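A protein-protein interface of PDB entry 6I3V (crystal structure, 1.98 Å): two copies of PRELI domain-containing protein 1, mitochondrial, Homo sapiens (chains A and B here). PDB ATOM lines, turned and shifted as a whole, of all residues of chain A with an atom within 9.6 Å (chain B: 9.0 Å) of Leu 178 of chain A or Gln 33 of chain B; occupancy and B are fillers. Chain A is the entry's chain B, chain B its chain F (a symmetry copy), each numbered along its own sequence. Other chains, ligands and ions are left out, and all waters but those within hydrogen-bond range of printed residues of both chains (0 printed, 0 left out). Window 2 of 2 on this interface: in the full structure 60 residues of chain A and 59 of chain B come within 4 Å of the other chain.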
ATOM      1  N   GLY A 170     -12.287 -29.594   9.816  1.00  0.00           N
ATOM      2  CA  GLY A 170     -11.639 -29.035   8.646  1.00  0.00           C
ATOM      3  C   GLY A 170     -10.292 -29.696   8.378  1.00  0.00           C
ATOM      4  O   GLY A 170      -9.964 -30.016   7.216  1.00  0.00           O
ATOM      5  N   PHE A 171      -9.485 -29.884   9.438  1.00  0.00           N
ATOM      6  CA  PHE A 171      -8.244 -30.640   9.341  1.00  0.00           C
ATOM      7  C   PHE A 171      -8.495 -32.036   8.752  1.00  0.00           C
ATOM      8  O   PHE A 171      -7.787 -32.473   7.842  1.00  0.00           O
ATOM      9  CB  PHE A 171      -7.590 -30.776  10.706  1.00  0.00           C
ATOM     10  CG  PHE A 171      -6.333 -29.925  10.904  1.00  0.00           C
ATOM     11  CD1 PHE A 171      -5.213 -30.104  10.104  1.00  0.00           C
ATOM     12  CD2 PHE A 171      -6.259 -29.006  11.967  1.00  0.00           C
ATOM     13  CE1 PHE A 171      -4.056 -29.362  10.298  1.00  0.00           C
ATOM     14  CE2 PHE A 171      -5.120 -28.235  12.170  1.00  0.00           C
ATOM     15  CZ  PHE A 171      -4.011 -28.445  11.373  1.00  0.00           C
ATOM     16  N   GLU A 172      -9.501 -32.753   9.263  1.00  0.00           N
ATOM     17  CA  GLU A 172      -9.743 -34.107   8.752  1.00  0.00           C
ATOM     18  C   GLU A 172     -10.129 -34.084   7.271  1.00  0.00           C
ATOM     19  O   GLU A 172      -9.688 -34.937   6.494  1.00  0.00           O
ATOM     20  CB  GLU A 172     -10.831 -34.795   9.588  1.00  0.00           C
ATOM     21  N   TYR A 173     -10.957 -33.120   6.886  1.00  0.00           N
ATOM     22  CA  TYR A 173     -11.340 -32.914   5.503  1.00  0.00           C
ATOM     23  C   TYR A 173     -10.116 -32.763   4.606  1.00  0.00           C
ATOM     24  O   TYR A 173      -9.995 -33.428   3.576  1.00  0.00           O
ATOM     25  CB  TYR A 173     -12.219 -31.654   5.413  1.00  0.00           C
ATOM     26  CG  TYR A 173     -12.717 -31.409   4.029  1.00  0.00           C
ATOM     27  CD1 TYR A 173     -13.809 -32.094   3.550  1.00  0.00           C
ATOM     28  CD2 TYR A 173     -12.071 -30.499   3.190  1.00  0.00           C
ATOM     29  CE1 TYR A 173     -14.259 -31.890   2.278  1.00  0.00           C
ATOM     30  CE2 TYR A 173     -12.504 -30.282   1.942  1.00  0.00           C
ATOM     31  CZ  TYR A 173     -13.604 -30.970   1.486  1.00  0.00           C
ATOM     32  OH  TYR A 173     -14.037 -30.728   0.215  1.00  0.00           O
ATOM     33  N   ILE A 174      -9.211 -31.850   4.968  1.00  0.00           N
ATOM     34  CA  ILE A 174      -8.085 -31.573   4.083  1.00  0.00           C
ATOM     35  C   ILE A 174      -7.067 -32.713   4.122  1.00  0.00           C
ATOM     36  O   ILE A 174      -6.491 -33.087   3.089  1.00  0.00           O
ATOM     37  CB  ILE A 174      -7.474 -30.197   4.445  1.00  0.00           C
ATOM     38  CG1 ILE A 174      -6.243 -29.897   3.592  1.00  0.00           C
ATOM     39  CG2 ILE A 174      -7.049 -30.193   5.879  1.00  0.00           C
ATOM     40  CD1 ILE A 174      -6.521 -29.814   2.108  1.00  0.00           C
ATOM     41  N   LEU A 175      -6.837 -33.320   5.292  1.00  0.00           N
ATOM     42  CA  LEU A 175      -5.959 -34.486   5.292  1.00  0.00           C
ATOM     43  C   LEU A 175      -6.521 -35.634   4.406  1.00  0.00           C
ATOM     44  O   LEU A 175      -5.751 -36.252   3.633  1.00  0.00           O
ATOM     45  CB  LEU A 175      -5.689 -34.972   6.714  1.00  0.00           C
ATOM     46  CG  LEU A 175      -4.842 -33.989   7.557  1.00  0.00           C
ATOM     47  CD1 LEU A 175      -5.043 -34.206   9.014  1.00  0.00           C
ATOM     48  CD2 LEU A 175      -3.394 -34.220   7.173  1.00  0.00           C
ATOM     49  N   ALA A 176      -7.833 -35.929   4.494  1.00  0.00           N
ATOM     50  CA  ALA A 176      -8.379 -37.005   3.636  1.00  0.00           C
ATOM     51  C   ALA A 176      -8.196 -36.652   2.173  1.00  0.00           C
ATOM     52  O   ALA A 176      -7.930 -37.517   1.338  1.00  0.00           O
ATOM     53  CB  ALA A 176      -9.862 -37.245   3.917  1.00  0.00           C
ATOM     54  N   LYS A 177      -8.371 -35.375   1.846  1.00  0.00           N
ATOM     55  CA  LYS A 177      -8.243 -34.913   0.483  1.00  0.00           C
ATOM     56  C   LYS A 177      -6.802 -34.993   0.011  1.00  0.00           C
ATOM     57  O   LYS A 177      -6.535 -35.393  -1.139  1.00  0.00           O
ATOM     58  CB  LYS A 177      -8.832 -33.505   0.395  1.00  0.00           C
ATOM     59  CG  LYS A 177      -8.539 -32.783  -0.864  1.00  0.00           C
ATOM     60  CD  LYS A 177      -8.854 -31.337  -0.679  1.00  0.00           C
ATOM     61  CE  LYS A 177     -10.177 -30.931  -1.239  1.00  0.00           C
ATOM     62  NZ  LYS A 177      -9.911 -30.382  -2.593  1.00  0.00           N
ATOM     63  N   LEU A 178      -5.860 -34.729   0.902  1.00  0.00           N
ATOM     64  CA  LEU A 178      -4.443 -34.786   0.560  1.00  0.00           C
ATOM     65  C   LEU A 178      -3.879 -36.205   0.513  1.00  0.00           C
ATOM     66  O   LEU A 178      -2.836 -36.407  -0.100  1.00  0.00           O
ATOM     67  CB  LEU A 178      -3.626 -33.951   1.564  1.00  0.00           C
ATOM     68  CG  LEU A 178      -3.638 -32.439   1.326  1.00  0.00           C
ATOM     69  CD1 LEU A 178      -3.095 -31.650   2.535  1.00  0.00           C
ATOM     70  CD2 LEU A 178      -2.790 -32.127   0.134  1.00  0.00           C
ATOM     71  N   GLN A 179      -4.506 -37.168   1.171  1.00  0.00           N
ATOM     72  CA  GLN A 179      -3.998 -38.527   1.239  1.00  0.00           C
ATOM     73  C   GLN A 179      -4.544 -39.250   0.008  1.00  0.00           C
ATOM     74  O   GLN A 179      -5.680 -39.728  -0.013  1.00  0.00           O
ATOM     75  CB  GLN A 179      -4.413 -39.171   2.550  1.00  0.00           C
ATOM     76  CG  GLN A 179      -4.187 -40.658   2.639  1.00  0.00           C
ATOM     77  CD  GLN A 179      -5.374 -41.356   3.278  1.00  0.00           C
ATOM     78  OE1 GLN A 179      -5.843 -40.938   4.343  1.00  0.00           O
ATOM     79  NE2 GLN A 179      -5.894 -42.407   2.613  1.00  0.00           N
ATOM     80  N   GLY A 180      -3.734 -39.295  -1.050  1.00  0.00           N
ATOM     81  CA  GLY A 180      -4.178 -39.757  -2.351  1.00  0.00           C
ATOM     82  C   GLY A 180      -4.279 -38.669  -3.399  1.00  0.00           C
ATOM     83  O   GLY A 180      -4.642 -38.972  -4.545  1.00  0.00           O
ATOM     84  N   GLU A 181      -3.983 -37.417  -3.039  1.00  0.00           N
ATOM     85  CA  GLU A 181      -3.879 -36.294  -3.977  1.00  0.00           C
ATOM     86  C   GLU A 181      -5.182 -36.007  -4.714  1.00  0.00           C
ATOM     87  O   GLU A 181      -5.208 -35.206  -5.649  1.00  0.00           O
ATOM     88  CB  GLU A 181      -2.758 -36.544  -4.998  1.00  0.00           C
ATOM     89  CG  GLU A 181      -1.362 -36.082  -4.563  1.00  0.00           C
ATOM     90  CD  GLU A 181      -0.618 -37.088  -3.694  1.00  0.00           C
ATOM     91  OE1 GLU A 181      -1.220 -38.106  -3.289  1.00  0.00           O
ATOM     92  OE2 GLU A 181       0.580 -36.857  -3.420  1.00  0.00           O
ATOM     93  N   SER B  22      -3.097 -38.888  11.380  1.00  0.00           N
ATOM     94  CA  SER B  22      -2.253 -38.554  10.238  1.00  0.00           C
ATOM     95  C   SER B  22      -0.862 -38.239  10.774  1.00  0.00           C
ATOM     96  O   SER B  22      -0.718 -37.908  11.945  1.00  0.00           O
ATOM     97  CB  SER B  22      -2.825 -37.368   9.447  1.00  0.00           C
ATOM     98  OG  SER B  22      -4.099 -37.735   8.932  1.00  0.00           O
ATOM     99  N   ASP B  25       4.151 -34.777   9.670  1.00  0.00           N
ATOM    100  CA  ASP B  25       4.483 -33.991   8.486  1.00  0.00           C
ATOM    101  C   ASP B  25       3.250 -33.685   7.632  1.00  0.00           C
ATOM    102  O   ASP B  25       3.191 -32.624   6.990  1.00  0.00           O
ATOM    103  CB  ASP B  25       5.550 -34.703   7.645  1.00  0.00           C
ATOM    104  CG  ASP B  25       5.143 -36.139   7.312  1.00  0.00           C
ATOM    105  OD1 ASP B  25       4.853 -36.919   8.241  1.00  0.00           O
ATOM    106  OD2 ASP B  25       5.075 -36.457   6.120  1.00  0.00           O
ATOM    107  N   GLN B  26       2.283 -34.618   7.540  1.00  0.00           N
ATOM    108  CA  GLN B  26       1.059 -34.325   6.794  1.00  0.00           C
ATOM    109  C   GLN B  26       0.247 -33.252   7.514  1.00  0.00           C
ATOM    110  O   GLN B  26      -0.339 -32.380   6.877  1.00  0.00           O
ATOM    111  CB  GLN B  26       0.196 -35.563   6.650  1.00  0.00           C
ATOM    112  CG  GLN B  26       0.924 -36.701   5.903  1.00  0.00           C
ATOM    113  CD  GLN B  26       0.206 -37.020   4.635  1.00  0.00           C
ATOM    114  OE1 GLN B  26      -0.277 -36.106   3.948  1.00  0.00           O
ATOM    115  NE2 GLN B  26       0.120 -38.321   4.294  1.00  0.00           N
ATOM    116  N   VAL B  27       0.152 -33.364   8.840  1.00  0.00           N
ATOM    117  CA  VAL B  27      -0.593 -32.366   9.604  1.00  0.00           C
ATOM    118  C   VAL B  27       0.070 -30.993   9.425  1.00  0.00           C
ATOM    119  O   VAL B  27      -0.607 -29.991   9.165  1.00  0.00           O
ATOM    120  CB  VAL B  27      -0.717 -32.805  11.090  1.00  0.00           C
ATOM    121  CG1 VAL B  27      -1.325 -31.653  11.973  1.00  0.00           C
ATOM    122  CG2 VAL B  27      -1.607 -34.067  11.255  1.00  0.00           C
ATOM    123  N   PHE B  28       1.412 -30.925   9.496  1.00  0.00           N
ATOM    124  CA  PHE B  28       2.029 -29.592   9.432  1.00  0.00           C
ATOM    125  C   PHE B  28       1.779 -28.994   8.061  1.00  0.00           C
ATOM    126  O   PHE B  28       1.525 -27.799   7.931  1.00  0.00           O
ATOM    127  CB  PHE B  28       3.543 -29.623   9.727  1.00  0.00           C
ATOM    128  CG  PHE B  28       3.905 -29.996  11.141  1.00  0.00           C
ATOM    129  CD1 PHE B  28       2.934 -30.423  12.039  1.00  0.00           C
ATOM    130  CD2 PHE B  28       5.215 -29.854  11.584  1.00  0.00           C
ATOM    131  CE1 PHE B  28       3.255 -30.735  13.352  1.00  0.00           C
ATOM    132  CE2 PHE B  28       5.545 -30.170  12.940  1.00  0.00           C
ATOM    133  CZ  PHE B  28       4.550 -30.615  13.810  1.00  0.00           C
ATOM    134  N   ALA B  29       1.817 -29.846   7.004  1.00  0.00           N
ATOM    135  CA  ALA B  29       1.528 -29.342   5.668  1.00  0.00           C
ATOM    136  C   ALA B  29       0.070 -28.918   5.554  1.00  0.00           C
ATOM    137  O   ALA B  29      -0.246 -27.868   4.982  1.00  0.00           O
ATOM    138  CB  ALA B  29       1.894 -30.421   4.590  1.00  0.00           C
ATOM    139  N   ALA B  30      -0.834 -29.706   6.115  1.00  0.00           N
ATOM    140  CA  ALA B  30      -2.250 -29.415   5.999  1.00  0.00           C
ATOM    141  C   ALA B  30      -2.618 -28.117   6.708  1.00  0.00           C
ATOM    142  O   ALA B  30      -3.591 -27.462   6.328  1.00  0.00           O
ATOM    143  CB  ALA B  30      -3.042 -30.557   6.604  1.00  0.00           C
ATOM    144  N   PHE B  31      -1.856 -27.763   7.762  1.00  0.00           N
ATOM    145  CA  PHE B  31      -2.101 -26.538   8.513  1.00  0.00           C
ATOM    146  C   PHE B  31      -2.186 -25.338   7.574  1.00  0.00           C
ATOM    147  O   PHE B  31      -3.027 -24.447   7.759  1.00  0.00           O
ATOM    148  CB  PHE B  31      -0.976 -26.378   9.534  1.00  0.00           C
ATOM    149  CG  PHE B  31      -1.137 -25.184  10.452  1.00  0.00           C
ATOM    150  CD1 PHE B  31      -2.077 -25.190  11.462  1.00  0.00           C
ATOM    151  CD2 PHE B  31      -0.274 -24.107  10.346  1.00  0.00           C
ATOM    152  CE1 PHE B  31      -2.158 -24.078  12.357  1.00  0.00           C
ATOM    153  CE2 PHE B  31      -0.365 -22.990  11.242  1.00  0.00           C
ATOM    154  CZ  PHE B  31      -1.325 -23.001  12.219  1.00  0.00           C
ATOM    155  N   TRP B  32      -1.332 -25.313   6.550  1.00  0.00           N
ATOM    156  CA  TRP B  32      -1.322 -24.203   5.619  1.00  0.00           C
ATOM    157  C   TRP B  32      -2.381 -24.313   4.545  1.00  0.00           C
ATOM    158  O   TRP B  32      -2.635 -23.313   3.880  1.00  0.00           O
ATOM    159  CB  TRP B  32       0.075 -24.060   4.999  1.00  0.00           C
ATOM    160  CG  TRP B  32       1.106 -23.871   6.120  1.00  0.00           C
ATOM    161  CD1 TRP B  32       2.110 -24.726   6.450  1.00  0.00           C
ATOM    162  CD2 TRP B  32       1.193 -22.768   7.049  1.00  0.00           C
ATOM    163  NE1 TRP B  32       2.840 -24.220   7.518  1.00  0.00           N
ATOM    164  CE2 TRP B  32       2.277 -23.039   7.924  1.00  0.00           C
ATOM    165  CE3 TRP B  32       0.419 -21.609   7.273  1.00  0.00           C
ATOM    166  CZ2 TRP B  32       2.643 -22.185   8.956  1.00  0.00           C
ATOM    167  CZ3 TRP B  32       0.804 -20.725   8.326  1.00  0.00           C
ATOM    168  CH2 TRP B  32       1.899 -21.030   9.139  1.00  0.00           C
ATOM    169  N   GLN B  33      -3.041 -25.467   4.385  1.00  0.00           N
ATOM    170  CA  GLN B  33      -3.947 -25.676   3.257  1.00  0.00           C
ATOM    171  C   GLN B  33      -5.369 -25.892   3.739  1.00  0.00           C
ATOM    172  O   GLN B  33      -6.247 -26.241   2.940  1.00  0.00           O
ATOM    173  CB  GLN B  33      -3.484 -26.899   2.430  1.00  0.00           C
ATOM    174  CG  GLN B  33      -2.094 -26.745   1.876  1.00  0.00           C
ATOM    175  CD  GLN B  33      -1.653 -27.938   1.029  1.00  0.00           C
ATOM    176  OE1 GLN B  33      -2.342 -28.319   0.111  1.00  0.00           O
ATOM    177  NE2 GLN B  33      -0.526 -28.528   1.357  1.00  0.00           N
ATOM    178  N   ARG B  34      -5.616 -25.749   5.033  1.00  0.00           N
ATOM    179  CA  ARG B  34      -6.913 -26.172   5.525  1.00  0.00           C
ATOM    180  C   ARG B  34      -8.036 -25.204   5.175  1.00  0.00           C
ATOM    181  O   ARG B  34      -9.203 -25.600   5.261  1.00  0.00           O
ATOM    182  CB  ARG B  34      -6.840 -26.398   7.022  1.00  0.00           C
ATOM    183  CG  ARG B  34      -6.585 -25.199   7.796  1.00  0.00           C
ATOM    184  CD  ARG B  34      -6.010 -25.644   9.146  1.00  0.00           C
ATOM    185  NE  ARG B  34      -5.472 -24.532   9.880  1.00  0.00           N
ATOM    186  CZ  ARG B  34      -6.178 -23.852  10.797  1.00  0.00           C
ATOM    187  NH1 ARG B  34      -7.433 -24.231  11.080  1.00  0.00           N
ATOM    188  NH2 ARG B  34      -5.641 -22.806  11.394  1.00  0.00           N
ATOM    189  N   TYR B  35      -7.735 -23.947   4.807  1.00  0.00           N
ATOM    190  CA  TYR B  35      -8.773 -23.060   4.303  1.00  0.00           C
ATOM    191  C   TYR B  35      -8.713 -22.952   2.769  1.00  0.00           C
ATOM    192  O   TYR B  35      -7.622 -22.826   2.227  1.00  0.00           O
ATOM    193  CB  TYR B  35      -8.647 -21.654   4.917  1.00  0.00           C
ATOM    194  CG  TYR B  35      -8.736 -21.640   6.449  1.00  0.00           C
ATOM    195  CD1 TYR B  35      -9.806 -22.221   7.119  1.00  0.00           C
ATOM    196  CD2 TYR B  35      -7.729 -21.073   7.208  1.00  0.00           C
ATOM    197  CE1 TYR B  35      -9.889 -22.202   8.539  1.00  0.00           C
ATOM    198  CE2 TYR B  35      -7.813 -21.013   8.599  1.00  0.00           C
ATOM    199  CZ  TYR B  35      -8.872 -21.599   9.254  1.00  0.00           C
ATOM    200  OH  TYR B  35      -8.922 -21.543  10.624  1.00  0.00           O
ATOM    201  N   PRO B  36      -9.882 -22.923   2.078  1.00  0.00           N
ATOM    202  CA  PRO B  36     -11.219 -23.026   2.689  1.00  0.00           C
ATOM    203  C   PRO B  36     -11.585 -24.506   2.869  1.00  0.00           C
ATOM    204  O   PRO B  36     -10.968 -25.372   2.252  1.00  0.00           O
ATOM    205  CB  PRO B  36     -12.122 -22.351   1.653  1.00  0.00           C
ATOM    206  CG  PRO B  36     -11.423 -22.837   0.285  1.00  0.00           C
ATOM    207  CD  PRO B  36      -9.946 -22.918   0.585  1.00  0.00           C
ATOM    208  N   ASN B  37     -12.573 -24.812   3.683  1.00  0.00           N
ATOM    209  CA  ASN B  37     -13.074 -26.182   3.744  1.00  0.00           C
ATOM    210  C   ASN B  37     -14.541 -26.065   4.110  1.00  0.00           C
ATOM    211  O   ASN B  37     -15.026 -24.964   4.396  1.00  0.00           O
ATOM    212  CB  ASN B  37     -12.260 -27.024   4.760  1.00  0.00           C
ATOM    213  CG  ASN B  37     -12.459 -26.523   6.222  1.00  0.00           C
ATOM    214  OD1 ASN B  37     -13.546 -26.654   6.792  1.00  0.00           O
ATOM    215  ND2 ASN B  37     -11.409 -25.950   6.803  1.00  0.00           N
ATOM    216  N   SER B  40     -15.481 -23.994   7.323  1.00  0.00           N
ATOM    217  CA  SER B  40     -14.768 -22.726   7.532  1.00  0.00           C
ATOM    218  C   SER B  40     -15.440 -21.545   6.829  1.00  0.00           C
ATOM    219  O   SER B  40     -14.763 -20.575   6.482  1.00  0.00           O
ATOM    220  CB  SER B  40     -13.311 -22.859   7.058  1.00  0.00           C
ATOM    221  OG  SER B  40     -13.160 -22.668   5.643  1.00  0.00           O
ATOM    222  N   GLU B  46      -7.557 -14.657   4.358  1.00  0.00           N
ATOM    223  CA  GLU B  46      -6.418 -15.353   4.928  1.00  0.00           C
ATOM    224  C   GLU B  46      -5.160 -14.798   4.305  1.00  0.00           C
ATOM    225  O   GLU B  46      -5.035 -14.766   3.070  1.00  0.00           O
ATOM    226  CB  GLU B  46      -6.532 -16.872   4.660  1.00  0.00           C
ATOM    227  CG  GLU B  46      -5.412 -17.664   5.242  1.00  0.00           C
ATOM    228  CD  GLU B  46      -5.181 -19.046   4.526  1.00  0.00           C
ATOM    229  OE1 GLU B  46      -5.211 -19.147   3.259  1.00  0.00           O
ATOM    230  OE2 GLU B  46      -4.949 -20.024   5.253  1.00  0.00           O
ATOM    231  N   ARG B  51       6.976 -13.887   7.619  1.00  0.00           N
ATOM    232  CA  ARG B  51       7.490 -15.255   7.614  1.00  0.00           C
ATOM    233  C   ARG B  51       9.009 -15.240   7.476  1.00  0.00           C
ATOM    234  O   ARG B  51       9.557 -14.485   6.676  1.00  0.00           O
ATOM    235  CB  ARG B  51       6.858 -16.088   6.486  1.00  0.00           C
ATOM    236  CG  ARG B  51       7.396 -17.531   6.388  1.00  0.00           C
ATOM    237  CD  ARG B  51       6.478 -18.357   5.461  1.00  0.00           C
ATOM    238  NE  ARG B  51       5.328 -18.910   6.195  1.00  0.00           N
ATOM    239  CZ  ARG B  51       4.166 -19.250   5.612  1.00  0.00           C
ATOM    240  NH1 ARG B  51       3.993 -19.052   4.303  1.00  0.00           N
ATOM    241  NH2 ARG B  51       3.179 -19.783   6.329  1.00  0.00           N
ATOM    242  N   ARG B  63      -0.040 -15.266  10.461  1.00  0.00           N
ATOM    243  CA  ARG B  63      -1.164 -15.357   9.533  1.00  0.00           C
ATOM    244  C   ARG B  63      -2.297 -14.483  10.047  1.00  0.00           C
ATOM    245  O   ARG B  63      -2.632 -14.520  11.239  1.00  0.00           O
ATOM    246  CB  ARG B  63      -1.626 -16.828   9.395  1.00  0.00           C
ATOM    247  CG  ARG B  63      -2.821 -17.083   8.519  1.00  0.00           C
ATOM    248  CD  ARG B  63      -2.841 -18.538   7.881  1.00  0.00           C
ATOM    249  NE  ARG B  63      -2.721 -19.593   8.883  1.00  0.00           N
ATOM    250  CZ  ARG B  63      -2.964 -20.883   8.615  1.00  0.00           C
ATOM    251  NH1 ARG B  63      -2.791 -21.830   9.565  1.00  0.00           N
ATOM    252  NH2 ARG B  63      -3.344 -21.237   7.370  1.00  0.00           N
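Of chain B, only Gln 33 (3.8 Å) comes within 4 Å of Leu 178 of chain A. Gln 33 of chain B touches just these residues of chain A: Ile 174 (3.7 Å) and Leu 178 (3.8 Å). Printed residues of chain A within 4 Å of Val 27 of chain B: Phe 171 (3.7 Å). Printed residues of chain A within 4 Å of Phe 31 of chain B: Phe 171. Phe 28 of chain B touches none of the printed residues of chain A.
Of the 18 printed residues of chain B, 8 touch a printed residue of chain A. Printed residues of chain B that touch a printed residue of chain A: Ser 22, Gln 26, Val 27, Ala 30, Phe 31, Gln 33, Arg 34 and Asn 37. Hydrophobic or aromatic side chains of chain A within 4 Å of the printed part of chain B: Phe 171, Tyr 173, Ile 174, Leu 175 and Leu 178. Among the printed residues, 10 pairs touch across the chains.
Among the printed residues, merely in contact across the chains: Gly 170 of chain A with Asn 37 of chain B (3.6 Å), Phe 171 of chain A with Val 27 of chain B (3.7 Å), Phe 171 of chain A with Phe 31 of chain B (3.7 Å), Tyr 173 of chain A with Asn 37 of chain B (3.8 Å), Ile 174 of chain A with Gln 33 of chain B (3.7 Å), Ile 174 of chain A with Arg 34 of chain B (3.97 Å), Leu 175 of chain A with Ser 22 of chain B (3.7 Å), Leu 175 of chain A with Gln 26 of chain B (3.6 Å), Leu 175 of chain A with Ala 30 of chain B (3.7 Å) and Leu 178 of chain A with Gln 33 of chain B (3.8 Å).
The backbone carbonyl oxygen (O) of Phe 31 of chain B lies within hydrogen-bond range of the guanidinium group (NE) of Arg 34 of chain B, 3.2 Å away. O of Phe 31 of chain B sits close to NH1 of Arg 63 of chain B, at 3.2 Å. The side-chain hydroxyl (OH) of Tyr 35 of chain B sits at hydrogen-bond distance from the guanidinium group (NH1) of Arg 34 of chain B (3.1 Å). The backbone carbonyl oxygen (O) of Arg 34 of chain B sits at hydrogen-bond distance from the side-chain amide nitrogen (ND2) of Asn 37 of chain B, 2.7 Å away. N of Asn 37 of chain B is in hydrogen-bond range of OG of Ser 40 of chain B, at 3.0 Å.
No position is printed for both chains. Of the 10 pairs that touch across the chains among the printed residues, none has its exchanged pair printed and touching as well.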
